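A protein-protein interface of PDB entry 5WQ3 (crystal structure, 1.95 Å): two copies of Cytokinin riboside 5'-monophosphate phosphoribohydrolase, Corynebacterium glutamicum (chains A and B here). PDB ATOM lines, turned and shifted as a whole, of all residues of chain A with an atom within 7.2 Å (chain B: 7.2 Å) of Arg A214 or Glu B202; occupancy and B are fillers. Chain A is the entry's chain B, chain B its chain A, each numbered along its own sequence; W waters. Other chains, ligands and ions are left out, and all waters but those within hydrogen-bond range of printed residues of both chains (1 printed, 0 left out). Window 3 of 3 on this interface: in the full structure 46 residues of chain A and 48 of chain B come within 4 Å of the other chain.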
ATOM      1  N   VAL A 208       5.636  10.367  17.293  1.00  0.00           N
ATOM      2  CA  VAL A 208       6.575  11.030  16.378  1.00  0.00           C
ATOM      3  C   VAL A 208       7.908  10.318  16.251  1.00  0.00           C
ATOM      4  O   VAL A 208       8.487  10.255  15.146  1.00  0.00           O
ATOM      5  CB  VAL A 208       6.820  12.479  16.713  1.00  0.00           C
ATOM      6  CG1 VAL A 208       7.844  13.067  15.755  1.00  0.00           C
ATOM      7  CG2 VAL A 208       5.568  13.245  16.582  1.00  0.00           C
ATOM      8  N   ASP A 209       8.404   9.767  17.356  1.00  0.00           N
ATOM      9  CA  ASP A 209       9.689   9.040  17.333  1.00  0.00           C
ATOM     10  C   ASP A 209       9.585   7.727  16.508  1.00  0.00           C
ATOM     11  O   ASP A 209      10.525   7.351  15.752  1.00  0.00           O
ATOM     12  CB  ASP A 209      10.171   8.811  18.772  1.00  0.00           C
ATOM     13  CG  ASP A 209      11.458   7.963  18.843  1.00  0.00           C
ATOM     14  OD1 ASP A 209      12.549   8.500  18.677  1.00  0.00           O
ATOM     15  OD2 ASP A 209      11.366   6.780  19.086  1.00  0.00           O
ATOM     16  N   TRP A 210       8.451   7.035  16.630  1.00  0.00           N
ATOM     17  CA  TRP A 210       8.188   5.802  15.846  1.00  0.00           C
ATOM     18  C   TRP A 210       8.107   6.124  14.350  1.00  0.00           C
ATOM     19  O   TRP A 210       8.787   5.514  13.534  1.00  0.00           O
ATOM     20  CB  TRP A 210       6.923   5.083  16.347  1.00  0.00           C
ATOM     21  CG  TRP A 210       6.592   3.847  15.581  1.00  0.00           C
ATOM     22  CD1 TRP A 210       7.251   2.638  15.635  1.00  0.00           C
ATOM     23  CD2 TRP A 210       5.529   3.675  14.644  1.00  0.00           C
ATOM     24  NE1 TRP A 210       6.661   1.741  14.791  1.00  0.00           N
ATOM     25  CE2 TRP A 210       5.609   2.353  14.160  1.00  0.00           C
ATOM     26  CE3 TRP A 210       4.514   4.505  14.170  1.00  0.00           C
ATOM     27  CZ2 TRP A 210       4.707   1.847  13.223  1.00  0.00           C
ATOM     28  CZ3 TRP A 210       3.634   4.014  13.238  1.00  0.00           C
ATOM     29  CH2 TRP A 210       3.726   2.699  12.770  1.00  0.00           C
ATOM     30  N   ILE A 211       7.332   7.142  14.010  1.00  0.00           N
ATOM     31  CA  ILE A 211       7.187   7.598  12.639  1.00  0.00           C
ATOM     32  C   ILE A 211       8.532   7.910  12.088  1.00  0.00           C
ATOM     33  O   ILE A 211       8.922   7.411  11.003  1.00  0.00           O
ATOM     34  CB  ILE A 211       6.321   8.875  12.577  1.00  0.00           C
ATOM     35  CG1 ILE A 211       4.855   8.514  12.814  1.00  0.00           C
ATOM     36  CG2 ILE A 211       6.490   9.619  11.242  1.00  0.00           C
ATOM     37  CD1 ILE A 211       4.006   9.762  12.995  1.00  0.00           C
ATOM     38  N   ARG A 212       9.224   8.750  12.827  1.00  0.00           N
ATOM     39  CA  ARG A 212      10.457   9.320  12.421  1.00  0.00           C
ATOM     40  C   ARG A 212      11.565   8.306  12.280  1.00  0.00           C
ATOM     41  O   ARG A 212      12.515   8.570  11.614  1.00  0.00           O
ATOM     42  CB  ARG A 212      10.869  10.407  13.370  1.00  0.00           C
ATOM     43  CG  ARG A 212      12.127  11.100  12.961  1.00  0.00           C
ATOM     44  CD  ARG A 212      12.469  12.168  13.957  1.00  0.00           C
ATOM     45  NE  ARG A 212      11.668  13.361  13.799  1.00  0.00           N
ATOM     46  CZ  ARG A 212      11.757  14.178  12.769  1.00  0.00           C
ATOM     47  NH1 ARG A 212      12.619  13.919  11.787  1.00  0.00           N
ATOM     48  NH2 ARG A 212      10.991  15.255  12.723  1.00  0.00           N
ATOM     49  N   HIS A 213      11.429   7.153  12.904  1.00  0.00           N
ATOM     50  CA  HIS A 213      12.459   6.142  12.851  1.00  0.00           C
ATOM     51  C   HIS A 213      12.058   4.844  12.136  1.00  0.00           C
ATOM     52  O   HIS A 213      12.774   4.361  11.294  1.00  0.00           O
ATOM     53  CB  HIS A 213      13.069   5.902  14.244  1.00  0.00           C
ATOM     54  CG  HIS A 213      13.942   7.030  14.704  1.00  0.00           C
ATOM     55  ND1 HIS A 213      13.708   7.732  15.863  1.00  0.00           N
ATOM     56  CD2 HIS A 213      15.012   7.621  14.124  1.00  0.00           C
ATOM     57  CE1 HIS A 213      14.609   8.685  15.986  1.00  0.00           C
ATOM     58  NE2 HIS A 213      15.413   8.637  14.944  1.00  0.00           N
ATOM     59  N   ARG A 214      10.917   4.295  12.462  1.00  0.00           N
ATOM     60  CA  ARG A 214      10.371   3.190  11.705  1.00  0.00           C
ATOM     61  C   ARG A 214      10.004   3.555  10.261  1.00  0.00           C
ATOM     62  O   ARG A 214      10.540   3.019   9.341  1.00  0.00           O
ATOM     63  CB  ARG A 214       9.135   2.649  12.397  1.00  0.00           C
ATOM     64  CG  ARG A 214       9.194   1.234  12.888  1.00  0.00           C
ATOM     65  CD  ARG A 214      10.213   0.382  12.177  1.00  0.00           C
ATOM     66  NE  ARG A 214      11.039  -0.315  13.134  1.00  0.00           N
ATOM     67  CZ  ARG A 214      11.507  -1.546  12.998  1.00  0.00           C
ATOM     68  NH1 ARG A 214      12.234  -2.053  13.962  1.00  0.00           N
ATOM     69  NH2 ARG A 214      11.255  -2.273  11.934  1.00  0.00           N
ATOM     70  N   LEU A 215       9.048   4.453  10.084  1.00  0.00           N
ATOM     71  CA  LEU A 215       8.543   4.798   8.774  1.00  0.00           C
ATOM     72  C   LEU A 215       9.557   5.448   7.838  1.00  0.00           C
ATOM     73  O   LEU A 215       9.605   5.106   6.693  1.00  0.00           O
ATOM     74  CB  LEU A 215       7.323   5.688   8.892  1.00  0.00           C
ATOM     75  CG  LEU A 215       6.121   5.204   9.665  1.00  0.00           C
ATOM     76  CD1 LEU A 215       4.848   5.906   9.301  1.00  0.00           C
ATOM     77  CD2 LEU A 215       5.957   3.721   9.642  1.00  0.00           C
ATOM     78  N   VAL A 216      10.321   6.407   8.333  1.00  0.00           N
ATOM     79  CA  VAL A 216      11.358   7.050   7.547  1.00  0.00           C
ATOM     80  C   VAL A 216      12.431   6.029   7.212  1.00  0.00           C
ATOM     81  O   VAL A 216      12.826   5.940   6.073  1.00  0.00           O
ATOM     82  CB  VAL A 216      11.955   8.250   8.297  1.00  0.00           C
ATOM     83  CG1 VAL A 216      13.239   8.756   7.626  1.00  0.00           C
ATOM     84  CG2 VAL A 216      10.908   9.366   8.448  1.00  0.00           C
ATOM     85  N   GLU A 217      12.873   5.215   8.169  1.00  0.00           N
ATOM     86  CA  GLU A 217      14.047   4.330   7.928  1.00  0.00           C
ATOM     87  C   GLU A 217      13.715   3.206   6.999  1.00  0.00           C
ATOM     88  O   GLU A 217      14.546   2.793   6.197  1.00  0.00           O
ATOM     89  CB  GLU A 217      14.628   3.720   9.222  1.00  0.00           C
ATOM     90  CG  GLU A 217      15.651   4.614   9.911  1.00  0.00           C
ATOM     91  CD  GLU A 217      16.290   3.976  11.143  1.00  0.00           C
ATOM     92  OE1 GLU A 217      15.612   3.224  11.887  1.00  0.00           O
ATOM     93  OE2 GLU A 217      17.493   4.218  11.353  1.00  0.00           O
ATOM     94  N   GLU A 218      12.502   2.683   7.126  1.00  0.00           N
ATOM     95  CA  GLU A 218      12.051   1.676   6.221  1.00  0.00           C
ATOM     96  C   GLU A 218      11.591   2.248   4.893  1.00  0.00           C
ATOM     97  O   GLU A 218      11.168   1.508   4.044  1.00  0.00           O
ATOM     98  CB  GLU A 218      10.980   0.830   6.861  1.00  0.00           C
ATOM     99  CG  GLU A 218      11.534   0.124   8.081  1.00  0.00           C
ATOM    100  CD  GLU A 218      10.907  -1.228   8.341  1.00  0.00           C
ATOM    101  OE1 GLU A 218      10.567  -1.496   9.501  1.00  0.00           O
ATOM    102  OE2 GLU A 218      10.781  -2.032   7.395  1.00  0.00           O
ATOM    103  N   GLY A 219      11.686   3.543   4.726  1.00  0.00           N
ATOM    104  CA  GLY A 219      11.391   4.136   3.451  1.00  0.00           C
ATOM    105  C   GLY A 219       9.940   4.246   3.072  1.00  0.00           C
ATOM    106  O   GLY A 219       9.605   4.341   1.914  1.00  0.00           O
ATOM    107  N   MET A 220       9.090   4.269   4.066  1.00  0.00           N
ATOM    108  CA  MET A 220       7.675   4.367   3.851  1.00  0.00           C
ATOM    109  C   MET A 220       7.120   5.766   3.777  1.00  0.00           C
ATOM    110  O   MET A 220       6.063   5.964   3.276  1.00  0.00           O
ATOM    111  CB  MET A 220       6.967   3.568   4.883  1.00  0.00           C
ATOM    112  CG  MET A 220       6.678   2.223   4.301  1.00  0.00           C
ATOM    113  SD  MET A 220       6.796   0.959   5.471  1.00  0.00           S
ATOM    114  CE  MET A 220       5.573   1.456   6.583  1.00  0.00           C
ATOM    115  N   ILE A 221       7.876   6.716   4.269  1.00  0.00           N
ATOM    116  CA  ILE A 221       7.625   8.102   4.031  1.00  0.00           C
ATOM    117  C   ILE A 221       8.943   8.784   3.860  1.00  0.00           C
ATOM    118  O   ILE A 221       9.923   8.249   4.237  1.00  0.00           O
ATOM    119  CB  ILE A 221       6.864   8.766   5.186  1.00  0.00           C
ATOM    120  CG1 ILE A 221       7.734   8.837   6.445  1.00  0.00           C
ATOM    121  CG2 ILE A 221       5.529   8.093   5.378  1.00  0.00           C
ATOM    122  CD1 ILE A 221       7.085   9.468   7.656  1.00  0.00           C
ATOM    123  N   TYR B  85       8.585  -8.234   3.487  1.00  0.00           N
ATOM    124  CA  TYR B  85       7.182  -7.838   3.611  1.00  0.00           C
ATOM    125  C   TYR B  85       6.340  -8.172   2.352  1.00  0.00           C
ATOM    126  O   TYR B  85       5.207  -8.659   2.463  1.00  0.00           O
ATOM    127  CB  TYR B  85       7.060  -6.357   3.921  1.00  0.00           C
ATOM    128  CG  TYR B  85       7.747  -5.835   5.145  1.00  0.00           C
ATOM    129  CD1 TYR B  85       8.086  -6.663   6.248  1.00  0.00           C
ATOM    130  CD2 TYR B  85       8.043  -4.476   5.219  1.00  0.00           C
ATOM    131  CE1 TYR B  85       8.707  -6.123   7.382  1.00  0.00           C
ATOM    132  CE2 TYR B  85       8.668  -3.922   6.322  1.00  0.00           C
ATOM    133  CZ  TYR B  85       8.992  -4.724   7.395  1.00  0.00           C
ATOM    134  OH  TYR B  85       9.612  -4.084   8.436  1.00  0.00           O
ATOM    135  N   ILE B 199       0.403  -7.145  10.728  1.00  0.00           N
ATOM    136  CA  ILE B 199       1.500  -8.022  10.386  1.00  0.00           C
ATOM    137  C   ILE B 199       2.856  -7.328  10.445  1.00  0.00           C
ATOM    138  O   ILE B 199       3.080  -6.382   9.759  1.00  0.00           O
ATOM    139  CB  ILE B 199       1.361  -8.626   8.978  1.00  0.00           C
ATOM    140  CG1 ILE B 199       0.017  -9.311   8.779  1.00  0.00           C
ATOM    141  CG2 ILE B 199       2.529  -9.553   8.655  1.00  0.00           C
ATOM    142  CD1 ILE B 199      -0.211 -10.500   9.638  1.00  0.00           C
ATOM    143  N   GLY B 200       3.761  -7.864  11.253  1.00  0.00           N
ATOM    144  CA  GLY B 200       5.134  -7.358  11.375  1.00  0.00           C
ATOM    145  C   GLY B 200       5.338  -6.865  12.786  1.00  0.00           C
ATOM    146  O   GLY B 200       5.023  -5.752  13.103  1.00  0.00           O
ATOM    147  N   THR B 201       5.852  -7.740  13.642  1.00  0.00           N
ATOM    148  CA  THR B 201       6.013  -7.459  15.061  1.00  0.00           C
ATOM    149  C   THR B 201       7.054  -6.418  15.285  1.00  0.00           C
ATOM    150  O   THR B 201       6.867  -5.547  16.039  1.00  0.00           O
ATOM    151  CB  THR B 201       6.440  -8.701  15.848  1.00  0.00           C
ATOM    152  OG1 THR B 201       7.422  -9.387  15.098  1.00  0.00           O
ATOM    153  CG2 THR B 201       5.293  -9.593  16.128  1.00  0.00           C
ATOM    154  N   GLU B 202       8.186  -6.556  14.631  1.00  0.00           N
ATOM    155  CA  GLU B 202       9.227  -5.563  14.723  1.00  0.00           C
ATOM    156  C   GLU B 202       8.674  -4.197  14.330  1.00  0.00           C
ATOM    157  O   GLU B 202       8.947  -3.210  14.950  1.00  0.00           O
ATOM    158  CB  GLU B 202      10.352  -5.919  13.781  1.00  0.00           C
ATOM    159  CG  GLU B 202      11.748  -5.666  14.284  1.00  0.00           C
ATOM    160  CD  GLU B 202      12.090  -6.463  15.505  1.00  0.00           C
ATOM    161  OE1 GLU B 202      11.256  -7.230  15.968  1.00  0.00           O
ATOM    162  OE2 GLU B 202      13.199  -6.295  16.015  1.00  0.00           O
ATOM    163  N   PHE B 203       7.915  -4.165  13.254  1.00  0.00           N
ATOM    164  CA  PHE B 203       7.475  -2.913  12.701  1.00  0.00           C
ATOM    165  C   PHE B 203       6.442  -2.204  13.555  1.00  0.00           C
ATOM    166  O   PHE B 203       6.506  -1.043  13.724  1.00  0.00           O
ATOM    167  CB  PHE B 203       6.978  -3.116  11.280  1.00  0.00           C
ATOM    168  CG  PHE B 203       6.406  -1.881  10.654  1.00  0.00           C
ATOM    169  CD1 PHE B 203       5.084  -1.568  10.808  1.00  0.00           C
ATOM    170  CD2 PHE B 203       7.196  -1.044   9.939  1.00  0.00           C
ATOM    171  CE1 PHE B 203       4.574  -0.457  10.239  1.00  0.00           C
ATOM    172  CE2 PHE B 203       6.695   0.079   9.377  1.00  0.00           C
ATOM    173  CZ  PHE B 203       5.381   0.370   9.528  1.00  0.00           C
ATOM    174  N   TRP B 204       5.505  -2.938  14.100  1.00  0.00           N
ATOM    175  CA  TRP B 204       4.325  -2.308  14.733  1.00  0.00           C
ATOM    176  C   TRP B 204       4.507  -2.044  16.219  1.00  0.00           C
ATOM    177  O   TRP B 204       3.819  -1.185  16.833  1.00  0.00           O
ATOM    178  CB  TRP B 204       3.084  -3.161  14.493  1.00  0.00           C
ATOM    179  CG  TRP B 204       2.593  -3.144  13.042  1.00  0.00           C
ATOM    180  CD1 TRP B 204       2.715  -4.147  12.106  1.00  0.00           C
ATOM    181  CD2 TRP B 204       1.865  -2.090  12.398  1.00  0.00           C
ATOM    182  NE1 TRP B 204       2.158  -3.756  10.909  1.00  0.00           N
ATOM    183  CE2 TRP B 204       1.620  -2.503  11.058  1.00  0.00           C
ATOM    184  CE3 TRP B 204       1.384  -0.840  12.819  1.00  0.00           C
ATOM    185  CZ2 TRP B 204       0.905  -1.704  10.136  1.00  0.00           C
ATOM    186  CZ3 TRP B 204       0.728  -0.031  11.896  1.00  0.00           C
ATOM    187  CH2 TRP B 204       0.489  -0.474  10.558  1.00  0.00           C
ATOM    188  N   ALA B 205       5.473  -2.759  16.812  1.00  0.00           N
ATOM    189  CA  ALA B 205       5.768  -2.656  18.258  1.00  0.00           C
ATOM    190  C   ALA B 205       5.771  -1.255  18.844  1.00  0.00           C
ATOM    191  O   ALA B 205       5.068  -0.973  19.824  1.00  0.00           O
ATOM    192  CB  ALA B 205       7.126  -3.319  18.532  1.00  0.00           C
ATOM    193  N   GLY B 206       6.552  -0.363  18.233  1.00  0.00           N
ATOM    194  CA  GLY B 206       6.636   1.031  18.705  1.00  0.00           C
ATOM    195  C   GLY B 206       5.304   1.726  18.793  1.00  0.00           C
ATOM    196  O   GLY B 206       5.022   2.453  19.764  1.00  0.00           O
ATOM    197  N   LEU B 207       4.476   1.543  17.755  1.00  0.00           N
ATOM    198  CA  LEU B 207       3.144   2.188  17.736  1.00  0.00           C
ATOM    199  C   LEU B 207       2.266   1.635  18.815  1.00  0.00           C
ATOM    200  O   LEU B 207       1.611   2.355  19.573  1.00  0.00           O
ATOM    201  CB  LEU B 207       2.399   1.958  16.376  1.00  0.00           C
ATOM    202  CG  LEU B 207       0.948   2.503  16.309  1.00  0.00           C
ATOM    203  CD1 LEU B 207       0.973   3.972  16.575  1.00  0.00           C
ATOM    204  CD2 LEU B 207       0.343   2.230  14.911  1.00  0.00           C
ATOM    205  N   VAL B 231      -1.359  -8.863  16.563  1.00  0.00           N
ATOM    206  CA  VAL B 231      -0.104  -8.444  15.982  1.00  0.00           C
ATOM    207  C   VAL B 231       0.728  -9.695  15.832  1.00  0.00           C
ATOM    208  O   VAL B 231       1.006 -10.331  16.843  1.00  0.00           O
ATOM    209  CB  VAL B 231       0.677  -7.453  16.909  1.00  0.00           C
ATOM    210  CG1 VAL B 231       1.954  -6.971  16.245  1.00  0.00           C
ATOM    211  CG2 VAL B 231      -0.197  -6.298  17.327  1.00  0.00           C
ATOM    212  N   THR B 232       1.170 -10.057  14.622  1.00  0.00           N
ATOM    213  CA  THR B 232       1.837 -11.320  14.469  1.00  0.00           C
ATOM    214  C   THR B 232       2.760 -11.314  13.276  1.00  0.00           C
ATOM    215  O   THR B 232       2.645 -10.480  12.370  1.00  0.00           O
ATOM    216  CB  THR B 232       0.821 -12.504  14.403  1.00  0.00           C
ATOM    217  OG1 THR B 232       1.529 -13.721  14.130  1.00  0.00           O
ATOM    218  CG2 THR B 232      -0.230 -12.300  13.301  1.00  0.00           C
ATOM    219  N   ASP B 233       3.683 -12.252  13.271  1.00  0.00           N
ATOM    220  CA  ASP B 233       4.423 -12.589  12.056  1.00  0.00           C
ATOM    221  C   ASP B 233       3.963 -13.883  11.428  1.00  0.00           C
ATOM    222  O   ASP B 233       4.552 -14.302  10.448  1.00  0.00           O
ATOM    223  CB  ASP B 233       5.915 -12.670  12.337  1.00  0.00           C
ATOM    224  CG  ASP B 233       6.431 -11.416  13.025  1.00  0.00           C
ATOM    225  OD1 ASP B 233       6.599 -10.365  12.352  1.00  0.00           O
ATOM    226  OD2 ASP B 233       6.595 -11.481  14.263  1.00  0.00           O
HETATM  227  O   HOH W   1       8.697  -0.521  15.738  1.00  0.00           O
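Printed residues of chain B within 4 Å of Trp A210: Phe B203, Gly B206 and Leu B207. Of chain B, only Glu B202 (3.6 Å) and Phe B203 (3.6 Å) come within 4 Å of Arg A214. Printed residues of chain B within 4 Å of Glu A218: Tyr B85 and Phe B203. Glu B202 touches just one residue of chain A: Arg A214 (3.6 Å). Of the printed residues of chain A, Gly B206 touches Trp A210. Thr B232 touches none of the printed residues of chain A. The nearest residue of chain B that does not touch Arg A214 is Tyr B85 (4.3 Å). The nearest residue of chain A that does not touch Glu B202 is Trp A210 (5.5 Å). The nearest printed residue of chain B that does not touch Leu A215 is Trp B204 (6.8 Å).
Water W1 lies within hydrogen-bond range of O of Glu B202 (2.8 Å), O of Phe B203 (3.0 Å), NE1 of Trp A210 (3.2 Å) and N of Gly B206 (3.3 Å).
OH of Tyr B85 sits at hydrogen-bond distance from OE2 of Glu A218 (2.6 Å). The indole nitrogen of Trp A210 sits at hydrogen-bond distance from the backbone carbonyl oxygen of Phe B203, 3.0 Å away.
No position is printed for both chains.
Among the printed residues, merely in contact across the chains: Met A220 with Phe B203, Leu A215 with Phe B203, Glu A218 with Phe B203, Trp A210 with Gly B206, Arg A214 with Phe B203, Arg A214 with Glu B202 and Trp A210 with Leu B207.
The side-chain carboxylate (OE1) of Glu A218 lies within salt-bridge range of the guanidinium group (NH2) of Arg A214, 2.6 Å away. N of Met A220 sits at hydrogen-bond distance from O of Leu A215 (2.8 Å). The backbone carbonyl oxygen of Leu A215 is in hydrogen-bond range of the backbone NH of Ile A221, at 3.4 Å.
Of the 13 printed residues of chain B, 5 touch a printed residue of chain A. Printed residues of chain B that touch a printed residue of chain A: Tyr B85, Glu B202, Phe B203, Gly B206 and Leu B207. Hydrophobic or aromatic side chains of chain B within 4 Å of the printed part of chain A: Tyr B85, Phe B203 and Leu B207. Of the 14 printed residues of chain A, 5 touch a printed residue of chain B. Hydrophobic or aromatic side chains of chain A that line the printed part of chain B: Trp A210, Leu A215 and Met A220.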
